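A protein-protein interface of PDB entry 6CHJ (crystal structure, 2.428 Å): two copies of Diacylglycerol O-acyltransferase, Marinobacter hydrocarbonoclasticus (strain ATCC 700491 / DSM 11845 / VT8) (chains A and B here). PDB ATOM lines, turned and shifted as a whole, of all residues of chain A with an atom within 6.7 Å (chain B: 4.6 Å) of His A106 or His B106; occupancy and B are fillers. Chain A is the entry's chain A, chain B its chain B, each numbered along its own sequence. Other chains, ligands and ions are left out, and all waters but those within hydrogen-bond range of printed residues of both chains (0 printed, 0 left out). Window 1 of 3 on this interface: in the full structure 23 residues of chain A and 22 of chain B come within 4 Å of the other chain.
His A106 touches just one residue of chain B: His B106.
His B106 touches just one residue of chain A: His A106.
Printed residues of chain A within 4 Å of Ala B102: Arg A83.
Of the printed residues of chain B, Arg A17 touches Leu B107 and Met B108.
Printed residues of chain B within 4 Å of Arg A83: Ala B102 (3.9 Å).
Arg A83 touches Ala B102, but with the chains exchanged Ala A102 does not touch Arg B83 (4.1 Å).
His B106 touches its own counterpart, His A106.
Positions printed for both chains: 22, 83, 102, 103, 104, 105, 106, 107, 108 and 133.
Of the 4 pairs that touch across the chains among the printed residues, 1 has its exchanged pair printed and touching as well.
The backbone carbonyl oxygen (O) of Ser A105 sits at hydrogen-bond distance from the guanidinium group (NH1) of Arg A17 (2.9 Å).
NH2 of Arg A83 is in salt-bridge range of OE2 of Glu A116 (3.4 Å).
O of Ala A102 lies within hydrogen-bond range of NE2 of His A106 (3.2 Å).
The side-chain amino group (NZ) of Lys A133 sits at hydrogen-bond distance from the backbone carbonyl oxygen (O) of His A106 (3.3 Å).
A ring nitrogen (NE2) of His B106 sits at hydrogen-bond distance from the backbone carbonyl oxygen (O) of Ala B102.
O of His B106 is in hydrogen-bond range of NZ of Lys B133 (3.1 Å).
Among the printed residues, pairs that only touch across the chains: His A106 with His B106 (3.2 Å), Arg A17 with Met B108 (3.7 Å), Arg A17 with Leu B107 (3.9 Å) and Arg A83 with Ala B102 (3.9 Å).
Of the 17 printed residues of chain A, 3 touch a printed residue of chain B.
Of the 10 printed residues of chain B, 4 touch a printed residue of chain A.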
ATOM      1  N   ARG A  17       3.059 -17.372  14.904  1.00  0.00           N
ATOM      2  CA  ARG A  17       2.094 -18.249  14.236  1.00  0.00           C
ATOM      3  C   ARG A  17       1.636 -17.679  12.900  1.00  0.00           C
ATOM      4  O   ARG A  17       1.345 -18.440  11.974  1.00  0.00           O
ATOM      5  CB  ARG A  17       0.876 -18.509  15.141  1.00  0.00           C
ATOM      6  CG  ARG A  17      -0.278 -19.353  14.473  1.00  0.00           C
ATOM      7  CD  ARG A  17       0.172 -20.793  14.091  1.00  0.00           C
ATOM      8  NE  ARG A  17      -0.724 -21.405  13.097  1.00  0.00           N
ATOM      9  CZ  ARG A  17      -0.401 -21.603  11.822  1.00  0.00           C
ATOM     10  NH1 ARG A  17       0.812 -21.257  11.379  1.00  0.00           N
ATOM     11  NH2 ARG A  17      -1.292 -22.130  10.985  1.00  0.00           N
ATOM     12  N   PRO A  20       5.449 -17.858   9.885  1.00  0.00           N
ATOM     13  CA  PRO A  20       6.566 -18.792   9.994  1.00  0.00           C
ATOM     14  C   PRO A  20       7.699 -18.294   9.115  1.00  0.00           C
ATOM     15  O   PRO A  20       7.475 -17.664   8.073  1.00  0.00           O
ATOM     16  CB  PRO A  20       5.980 -20.115   9.486  1.00  0.00           C
ATOM     17  CG  PRO A  20       4.460 -19.898   9.505  1.00  0.00           C
ATOM     18  CD  PRO A  20       4.302 -18.451   9.185  1.00  0.00           C
ATOM     19  N   HIS A  22      10.169 -20.126   7.564  1.00  0.00           N
ATOM     20  CA  HIS A  22      10.814 -21.190   6.814  1.00  0.00           C
ATOM     21  C   HIS A  22      10.624 -20.922   5.329  1.00  0.00           C
ATOM     22  O   HIS A  22       9.629 -20.318   4.920  1.00  0.00           O
ATOM     23  CB  HIS A  22      10.264 -22.572   7.198  1.00  0.00           C
ATOM     24  CG  HIS A  22       8.785 -22.701   7.008  1.00  0.00           C
ATOM     25  ND1 HIS A  22       7.902 -22.767   8.063  1.00  0.00           N
ATOM     26  CD2 HIS A  22       8.035 -22.758   5.881  1.00  0.00           C
ATOM     27  CE1 HIS A  22       6.669 -22.836   7.595  1.00  0.00           C
ATOM     28  NE2 HIS A  22       6.722 -22.841   6.273  1.00  0.00           N
ATOM     29  N   ARG A  83       9.244 -37.555   4.795  1.00  0.00           N
ATOM     30  CA  ARG A  83       7.881 -38.042   4.709  1.00  0.00           C
ATOM     31  C   ARG A  83       7.563 -38.435   3.272  1.00  0.00           C
ATOM     32  O   ARG A  83       8.136 -37.898   2.319  1.00  0.00           O
ATOM     33  CB  ARG A  83       6.895 -36.985   5.206  1.00  0.00           C
ATOM     34  CG  ARG A  83       6.763 -36.961   6.721  1.00  0.00           C
ATOM     35  CD  ARG A  83       6.096 -35.685   7.220  1.00  0.00           C
ATOM     36  NE  ARG A  83       6.947 -34.957   8.164  1.00  0.00           N
ATOM     37  CZ  ARG A  83       6.494 -34.110   9.089  1.00  0.00           C
ATOM     38  NH1 ARG A  83       5.190 -33.877   9.205  1.00  0.00           N
ATOM     39  NH2 ARG A  83       7.346 -33.495   9.900  1.00  0.00           N
ATOM     40  N   SER A 101       0.539 -25.585  -0.257  1.00  0.00           N
ATOM     41  CA  SER A 101      -0.034 -24.464   0.491  1.00  0.00           C
ATOM     42  C   SER A 101      -0.281 -24.854   1.944  1.00  0.00           C
ATOM     43  O   SER A 101       0.033 -24.088   2.862  1.00  0.00           O
ATOM     44  CB  SER A 101      -1.332 -23.977  -0.159  1.00  0.00           C
ATOM     45  OG  SER A 101      -1.164 -23.784  -1.551  1.00  0.00           O
ATOM     46  N   ALA A 102      -0.803 -26.067   2.166  1.00  0.00           N
ATOM     47  CA  ALA A 102      -1.069 -26.553   3.523  1.00  0.00           C
ATOM     48  C   ALA A 102       0.226 -26.807   4.296  1.00  0.00           C
ATOM     49  O   ALA A 102       0.381 -26.325   5.416  1.00  0.00           O
ATOM     50  CB  ALA A 102      -1.929 -27.831   3.472  1.00  0.00           C
ATOM     51  N   GLU A 103       1.158 -27.597   3.732  1.00  0.00           N
ATOM     52  CA  GLU A 103       2.415 -27.886   4.432  1.00  0.00           C
ATOM     53  C   GLU A 103       3.161 -26.609   4.780  1.00  0.00           C
ATOM     54  O   GLU A 103       3.716 -26.486   5.872  1.00  0.00           O
ATOM     55  CB  GLU A 103       3.341 -28.758   3.580  1.00  0.00           C
ATOM     56  CG  GLU A 103       3.140 -30.227   3.682  1.00  0.00           C
ATOM     57  CD  GLU A 103       2.762 -30.673   5.072  1.00  0.00           C
ATOM     58  OE1 GLU A 103       3.513 -30.382   6.027  1.00  0.00           O
ATOM     59  OE2 GLU A 103       1.699 -31.315   5.193  1.00  0.00           O
ATOM     60  N   HIS A 104       3.219 -25.665   3.843  1.00  0.00           N
ATOM     61  CA  HIS A 104       3.987 -24.446   4.046  1.00  0.00           C
ATOM     62  C   HIS A 104       3.442 -23.573   5.169  1.00  0.00           C
ATOM     63  O   HIS A 104       4.167 -22.681   5.633  1.00  0.00           O
ATOM     64  CB  HIS A 104       4.047 -23.640   2.752  1.00  0.00           C
ATOM     65  CG  HIS A 104       5.219 -22.730   2.695  1.00  0.00           C
ATOM     66  ND1 HIS A 104       6.486 -23.182   2.398  1.00  0.00           N
ATOM     67  CD2 HIS A 104       5.336 -21.405   2.962  1.00  0.00           C
ATOM     68  CE1 HIS A 104       7.333 -22.171   2.470  1.00  0.00           C
ATOM     69  NE2 HIS A 104       6.659 -21.083   2.803  1.00  0.00           N
ATOM     70  N   SER A 105       2.200 -23.807   5.622  1.00  0.00           N
ATOM     71  CA  SER A 105       1.608 -23.025   6.707  1.00  0.00           C
ATOM     72  C   SER A 105       2.029 -23.503   8.091  1.00  0.00           C
ATOM     73  O   SER A 105       1.817 -22.774   9.066  1.00  0.00           O
ATOM     74  CB  SER A 105       0.074 -23.074   6.643  1.00  0.00           C
ATOM     75  OG  SER A 105      -0.397 -22.937   5.311  1.00  0.00           O
ATOM     76  N   HIS A 106       2.590 -24.705   8.210  1.00  0.00           N
ATOM     77  CA  HIS A 106       2.823 -25.322   9.516  1.00  0.00           C
ATOM     78  C   HIS A 106       4.188 -24.908  10.061  1.00  0.00           C
ATOM     79  O   HIS A 106       5.214 -25.124   9.405  1.00  0.00           O
ATOM     80  CB  HIS A 106       2.741 -26.853   9.428  1.00  0.00           C
ATOM     81  CG  HIS A 106       1.463 -27.387   8.827  1.00  0.00           C
ATOM     82  ND1 HIS A 106       0.215 -26.841   9.080  1.00  0.00           N
ATOM     83  CD2 HIS A 106       1.248 -28.445   8.003  1.00  0.00           C
ATOM     84  CE1 HIS A 106      -0.706 -27.527   8.430  1.00  0.00           C
ATOM     85  NE2 HIS A 106      -0.106 -28.499   7.759  1.00  0.00           N
ATOM     86  N   LEU A 107       4.207 -24.336  11.265  1.00  0.00           N
ATOM     87  CA  LEU A 107       5.474 -24.034  11.924  1.00  0.00           C
ATOM     88  C   LEU A 107       6.336 -25.284  12.045  1.00  0.00           C
ATOM     89  O   LEU A 107       5.831 -26.402  12.213  1.00  0.00           O
ATOM     90  CB  LEU A 107       5.247 -23.467  13.318  1.00  0.00           C
ATOM     91  CG  LEU A 107       4.811 -22.017  13.507  1.00  0.00           C
ATOM     92  CD1 LEU A 107       4.691 -21.751  15.008  1.00  0.00           C
ATOM     93  CD2 LEU A 107       5.761 -21.024  12.841  1.00  0.00           C
ATOM     94  N   MET A 108       7.644 -25.085  11.996  1.00  0.00           N
ATOM     95  CA  MET A 108       8.584 -26.173  12.182  1.00  0.00           C
ATOM     96  C   MET A 108       8.900 -26.336  13.675  1.00  0.00           C
ATOM     97  O   MET A 108       8.720 -25.419  14.475  1.00  0.00           O
ATOM     98  CB  MET A 108       9.851 -25.919  11.362  1.00  0.00           C
ATOM     99  CG  MET A 108       9.593 -25.716   9.876  1.00  0.00           C
ATOM    100  SD  MET A 108      11.031 -26.016   8.812  1.00  0.00           S
ATOM    101  CE  MET A 108      11.158 -27.796   8.999  1.00  0.00           C
ATOM    102  N   ASP A 109       9.342 -27.530  14.057  1.00  0.00           N
ATOM    103  CA  ASP A 109       9.624 -27.820  15.460  1.00  0.00           C
ATOM    104  C   ASP A 109      11.072 -27.435  15.733  1.00  0.00           C
ATOM    105  O   ASP A 109      11.982 -27.900  15.041  1.00  0.00           O
ATOM    106  CB  ASP A 109       9.369 -29.298  15.766  1.00  0.00           C
ATOM    107  CG  ASP A 109       9.271 -29.614  17.274  1.00  0.00           C
ATOM    108  OD1 ASP A 109       9.358 -28.709  18.159  1.00  0.00           O
ATOM    109  OD2 ASP A 109       9.081 -30.829  17.558  1.00  0.00           O
ATOM    110  N   GLU A 116      12.694 -30.521   6.358  1.00  0.00           N
ATOM    111  CA  GLU A 116      11.732 -31.548   6.006  1.00  0.00           C
ATOM    112  C   GLU A 116      11.780 -31.765   4.495  1.00  0.00           C
ATOM    113  O   GLU A 116      11.874 -30.796   3.726  1.00  0.00           O
ATOM    114  CB  GLU A 116      10.314 -31.147   6.427  1.00  0.00           C
ATOM    115  CG  GLU A 116       9.999 -31.183   7.904  1.00  0.00           C
ATOM    116  CD  GLU A 116       8.599 -30.649   8.214  1.00  0.00           C
ATOM    117  OE1 GLU A 116       7.751 -30.535   7.291  1.00  0.00           O
ATOM    118  OE2 GLU A 116       8.339 -30.326   9.391  1.00  0.00           O
ATOM    119  N   LYS A 133      11.349 -28.165   2.803  1.00  0.00           N
ATOM    120  CA  LYS A 133      11.069 -27.037   3.677  1.00  0.00           C
ATOM    121  C   LYS A 133      12.224 -26.968   4.650  1.00  0.00           C
ATOM    122  O   LYS A 133      12.525 -27.971   5.302  1.00  0.00           O
ATOM    123  CB  LYS A 133       9.750 -27.255   4.423  1.00  0.00           C
ATOM    124  CG  LYS A 133       9.424 -26.272   5.520  1.00  0.00           C
ATOM    125  CD  LYS A 133       8.465 -26.944   6.511  1.00  0.00           C
ATOM    126  CE  LYS A 133       7.130 -26.223   6.606  1.00  0.00           C
ATOM    127  NZ  LYS A 133       6.048 -27.172   6.992  1.00  0.00           N
ATOM    128  N   GLY A 237      -1.560 -17.199   9.427  1.00  0.00           N
ATOM    129  CA  GLY A 237      -0.535 -18.174   9.100  1.00  0.00           C
ATOM    130  C   GLY A 237      -0.902 -19.162   8.004  1.00  0.00           C
ATOM    131  O   GLY A 237      -0.033 -19.917   7.539  1.00  0.00           O
ATOM    132  N   ARG A 239      -1.659 -20.287   4.252  1.00  0.00           N
ATOM    133  CA  ARG A 239      -0.939 -19.911   3.046  1.00  0.00           C
ATOM    134  C   ARG A 239      -1.649 -20.404   1.799  1.00  0.00           C
ATOM    135  O   ARG A 239      -2.361 -21.418   1.825  1.00  0.00           O
ATOM    136  CB  ARG A 239       0.481 -20.493   3.046  1.00  0.00           C
ATOM    137  CG  ARG A 239       1.374 -19.883   4.073  1.00  0.00           C
ATOM    138  CD  ARG A 239       1.700 -18.452   3.705  1.00  0.00           C
ATOM    139  NE  ARG A 239       2.448 -17.794   4.770  1.00  0.00           N
ATOM    140  CZ  ARG A 239       1.890 -17.092   5.753  1.00  0.00           C
ATOM    141  NH1 ARG A 239       0.567 -16.955   5.807  1.00  0.00           N
ATOM    142  NH2 ARG A 239       2.661 -16.534   6.679  1.00  0.00           N
ATOM    143  N   HIS B  22      -5.580 -28.602  20.762  1.00  0.00           N
ATOM    144  CA  HIS B  22      -6.736 -29.046  20.003  1.00  0.00           C
ATOM    145  C   HIS B  22      -6.963 -30.536  20.248  1.00  0.00           C
ATOM    146  O   HIS B  22      -6.020 -31.292  20.481  1.00  0.00           O
ATOM    147  CB  HIS B  22      -6.557 -28.771  18.505  1.00  0.00           C
ATOM    148  CG  HIS B  22      -5.350 -29.424  17.894  1.00  0.00           C
ATOM    149  ND1 HIS B  22      -4.171 -28.747  17.660  1.00  0.00           N
ATOM    150  CD2 HIS B  22      -5.149 -30.689  17.450  1.00  0.00           C
ATOM    151  CE1 HIS B  22      -3.290 -29.568  17.120  1.00  0.00           C
ATOM    152  NE2 HIS B  22      -3.856 -30.756  16.987  1.00  0.00           N
ATOM    153  N   ARG B  83     -10.723 -30.552   3.835  1.00  0.00           N
ATOM    154  CA  ARG B  83      -9.563 -30.947   3.052  1.00  0.00           C
ATOM    155  C   ARG B  83      -9.698 -32.382   2.584  1.00  0.00           C
ATOM    156  O   ARG B  83     -10.131 -33.262   3.338  1.00  0.00           O
ATOM    157  CB  ARG B  83      -8.268 -30.778   3.850  1.00  0.00           C
ATOM    158  CG  ARG B  83      -8.066 -29.344   4.257  1.00  0.00           C
ATOM    159  CD  ARG B  83      -6.680 -29.036   4.689  1.00  0.00           C
ATOM    160  NE  ARG B  83      -6.685 -27.767   5.412  1.00  0.00           N
ATOM    161  CZ  ARG B  83      -5.746 -27.406   6.272  1.00  0.00           C
ATOM    162  NH1 ARG B  83      -4.733 -28.225   6.504  1.00  0.00           N
ATOM    163  NH2 ARG B  83      -5.824 -26.244   6.908  1.00  0.00           N
ATOM    164  N   ALA B 102       1.043 -36.760  11.911  1.00  0.00           N
ATOM    165  CA  ALA B 102       1.509 -35.523  11.283  1.00  0.00           C
ATOM    166  C   ALA B 102       0.477 -34.408  11.410  1.00  0.00           C
ATOM    167  O   ALA B 102       0.801 -33.286  11.812  1.00  0.00           O
ATOM    168  CB  ALA B 102       1.827 -35.778   9.802  1.00  0.00           C
ATOM    169  N   GLU B 103      -0.776 -34.691  11.055  1.00  0.00           N
ATOM    170  CA  GLU B 103      -1.770 -33.627  11.035  1.00  0.00           C
ATOM    171  C   GLU B 103      -2.113 -33.145  12.452  1.00  0.00           C
ATOM    172  O   GLU B 103      -2.329 -31.948  12.662  1.00  0.00           O
ATOM    173  CB  GLU B 103      -3.016 -34.100  10.284  1.00  0.00           C
ATOM    174  CG  GLU B 103      -3.930 -32.967   9.880  1.00  0.00           C
ATOM    175  CD  GLU B 103      -3.206 -31.865   9.090  1.00  0.00           C
ATOM    176  OE1 GLU B 103      -2.445 -32.200   8.158  1.00  0.00           O
ATOM    177  OE2 GLU B 103      -3.401 -30.666   9.419  1.00  0.00           O
ATOM    178  N   HIS B 104      -2.131 -34.050  13.444  1.00  0.00           N
ATOM    179  CA  HIS B 104      -2.454 -33.661  14.817  1.00  0.00           C
ATOM    180  C   HIS B 104      -1.349 -32.808  15.458  1.00  0.00           C
ATOM    181  O   HIS B 104      -1.640 -32.028  16.370  1.00  0.00           O
ATOM    182  CB  HIS B 104      -2.719 -34.917  15.663  1.00  0.00           C
ATOM    183  CG  HIS B 104      -3.494 -34.647  16.913  1.00  0.00           C
ATOM    184  ND1 HIS B 104      -4.848 -34.383  16.905  1.00  0.00           N
ATOM    185  CD2 HIS B 104      -3.098 -34.567  18.209  1.00  0.00           C
ATOM    186  CE1 HIS B 104      -5.256 -34.148  18.141  1.00  0.00           C
ATOM    187  NE2 HIS B 104      -4.218 -34.270  18.952  1.00  0.00           N
ATOM    188  N   SER B 105      -0.090 -32.945  15.009  1.00  0.00           N
ATOM    189  CA  SER B 105       1.007 -32.087  15.470  1.00  0.00           C
ATOM    190  C   SER B 105       0.784 -30.594  15.199  1.00  0.00           C
ATOM    191  O   SER B 105       1.335 -29.760  15.916  1.00  0.00           O
ATOM    192  CB  SER B 105       2.305 -32.489  14.780  1.00  0.00           C
ATOM    193  OG  SER B 105       2.577 -33.858  14.956  1.00  0.00           O
ATOM    194  N   HIS B 106       0.058 -30.231  14.141  1.00  0.00           N
ATOM    195  CA  HIS B 106       0.089 -28.857  13.645  1.00  0.00           C
ATOM    196  C   HIS B 106      -0.838 -27.946  14.436  1.00  0.00           C
ATOM    197  O   HIS B 106      -2.035 -28.233  14.578  1.00  0.00           O
ATOM    198  CB  HIS B 106      -0.312 -28.811  12.170  1.00  0.00           C
ATOM    199  CG  HIS B 106       0.530 -29.679  11.294  1.00  0.00           C
ATOM    200  ND1 HIS B 106       1.900 -29.766  11.426  1.00  0.00           N
ATOM    201  CD2 HIS B 106       0.191 -30.529  10.295  1.00  0.00           C
ATOM    202  CE1 HIS B 106       2.371 -30.619  10.535  1.00  0.00           C
ATOM    203  NE2 HIS B 106       1.353 -31.102   9.843  1.00  0.00           N
ATOM    204  N   LEU B 107      -0.271 -26.839  14.926  1.00  0.00           N
ATOM    205  CA  LEU B 107      -1.044 -25.725  15.470  1.00  0.00           C
ATOM    206  C   LEU B 107      -2.138 -25.278  14.514  1.00  0.00           C
ATOM    207  O   LEU B 107      -1.930 -25.190  13.300  1.00  0.00           O
ATOM    208  CB  LEU B 107      -0.127 -24.533  15.737  1.00  0.00           C
ATOM    209  CG  LEU B 107       0.696 -24.531  17.017  1.00  0.00           C
ATOM    210  CD1 LEU B 107       1.416 -23.204  17.125  1.00  0.00           C
ATOM    211  CD2 LEU B 107      -0.151 -24.816  18.274  1.00  0.00           C
ATOM    212  N   MET B 108      -3.301 -24.965  15.066  1.00  0.00           N
ATOM    213  CA  MET B 108      -4.358 -24.393  14.252  1.00  0.00           C
ATOM    214  C   MET B 108      -4.216 -22.878  14.208  1.00  0.00           C
ATOM    215  O   MET B 108      -3.657 -22.258  15.106  1.00  0.00           O
ATOM    216  CB  MET B 108      -5.739 -24.762  14.788  1.00  0.00           C
ATOM    217  CG  MET B 108      -5.858 -26.162  15.261  1.00  0.00           C
ATOM    218  SD  MET B 108      -7.545 -26.642  15.636  1.00  0.00           S
ATOM    219  CE  MET B 108      -8.228 -26.537  13.966  1.00  0.00           C
ATOM    220  N   LYS B 133     -10.420 -32.136  13.559  1.00  0.00           N
ATOM    221  CA  LYS B 133      -9.562 -31.445  14.520  1.00  0.00           C
ATOM    222  C   LYS B 133     -10.315 -30.214  14.992  1.00  0.00           C
ATOM    223  O   LYS B 133     -10.675 -29.364  14.169  1.00  0.00           O
ATOM    224  CB  LYS B 133      -8.227 -31.046  13.862  1.00  0.00           C
ATOM    225  CG  LYS B 133      -7.243 -30.297  14.748  1.00  0.00           C
ATOM    226  CD  LYS B 133      -6.168 -29.539  13.969  1.00  0.00           C
ATOM    227  CE  LYS B 133      -5.434 -30.402  12.944  1.00  0.00           C
ATOM    228  NZ  LYS B 133      -3.962 -30.106  13.002  1.00  0.00           N
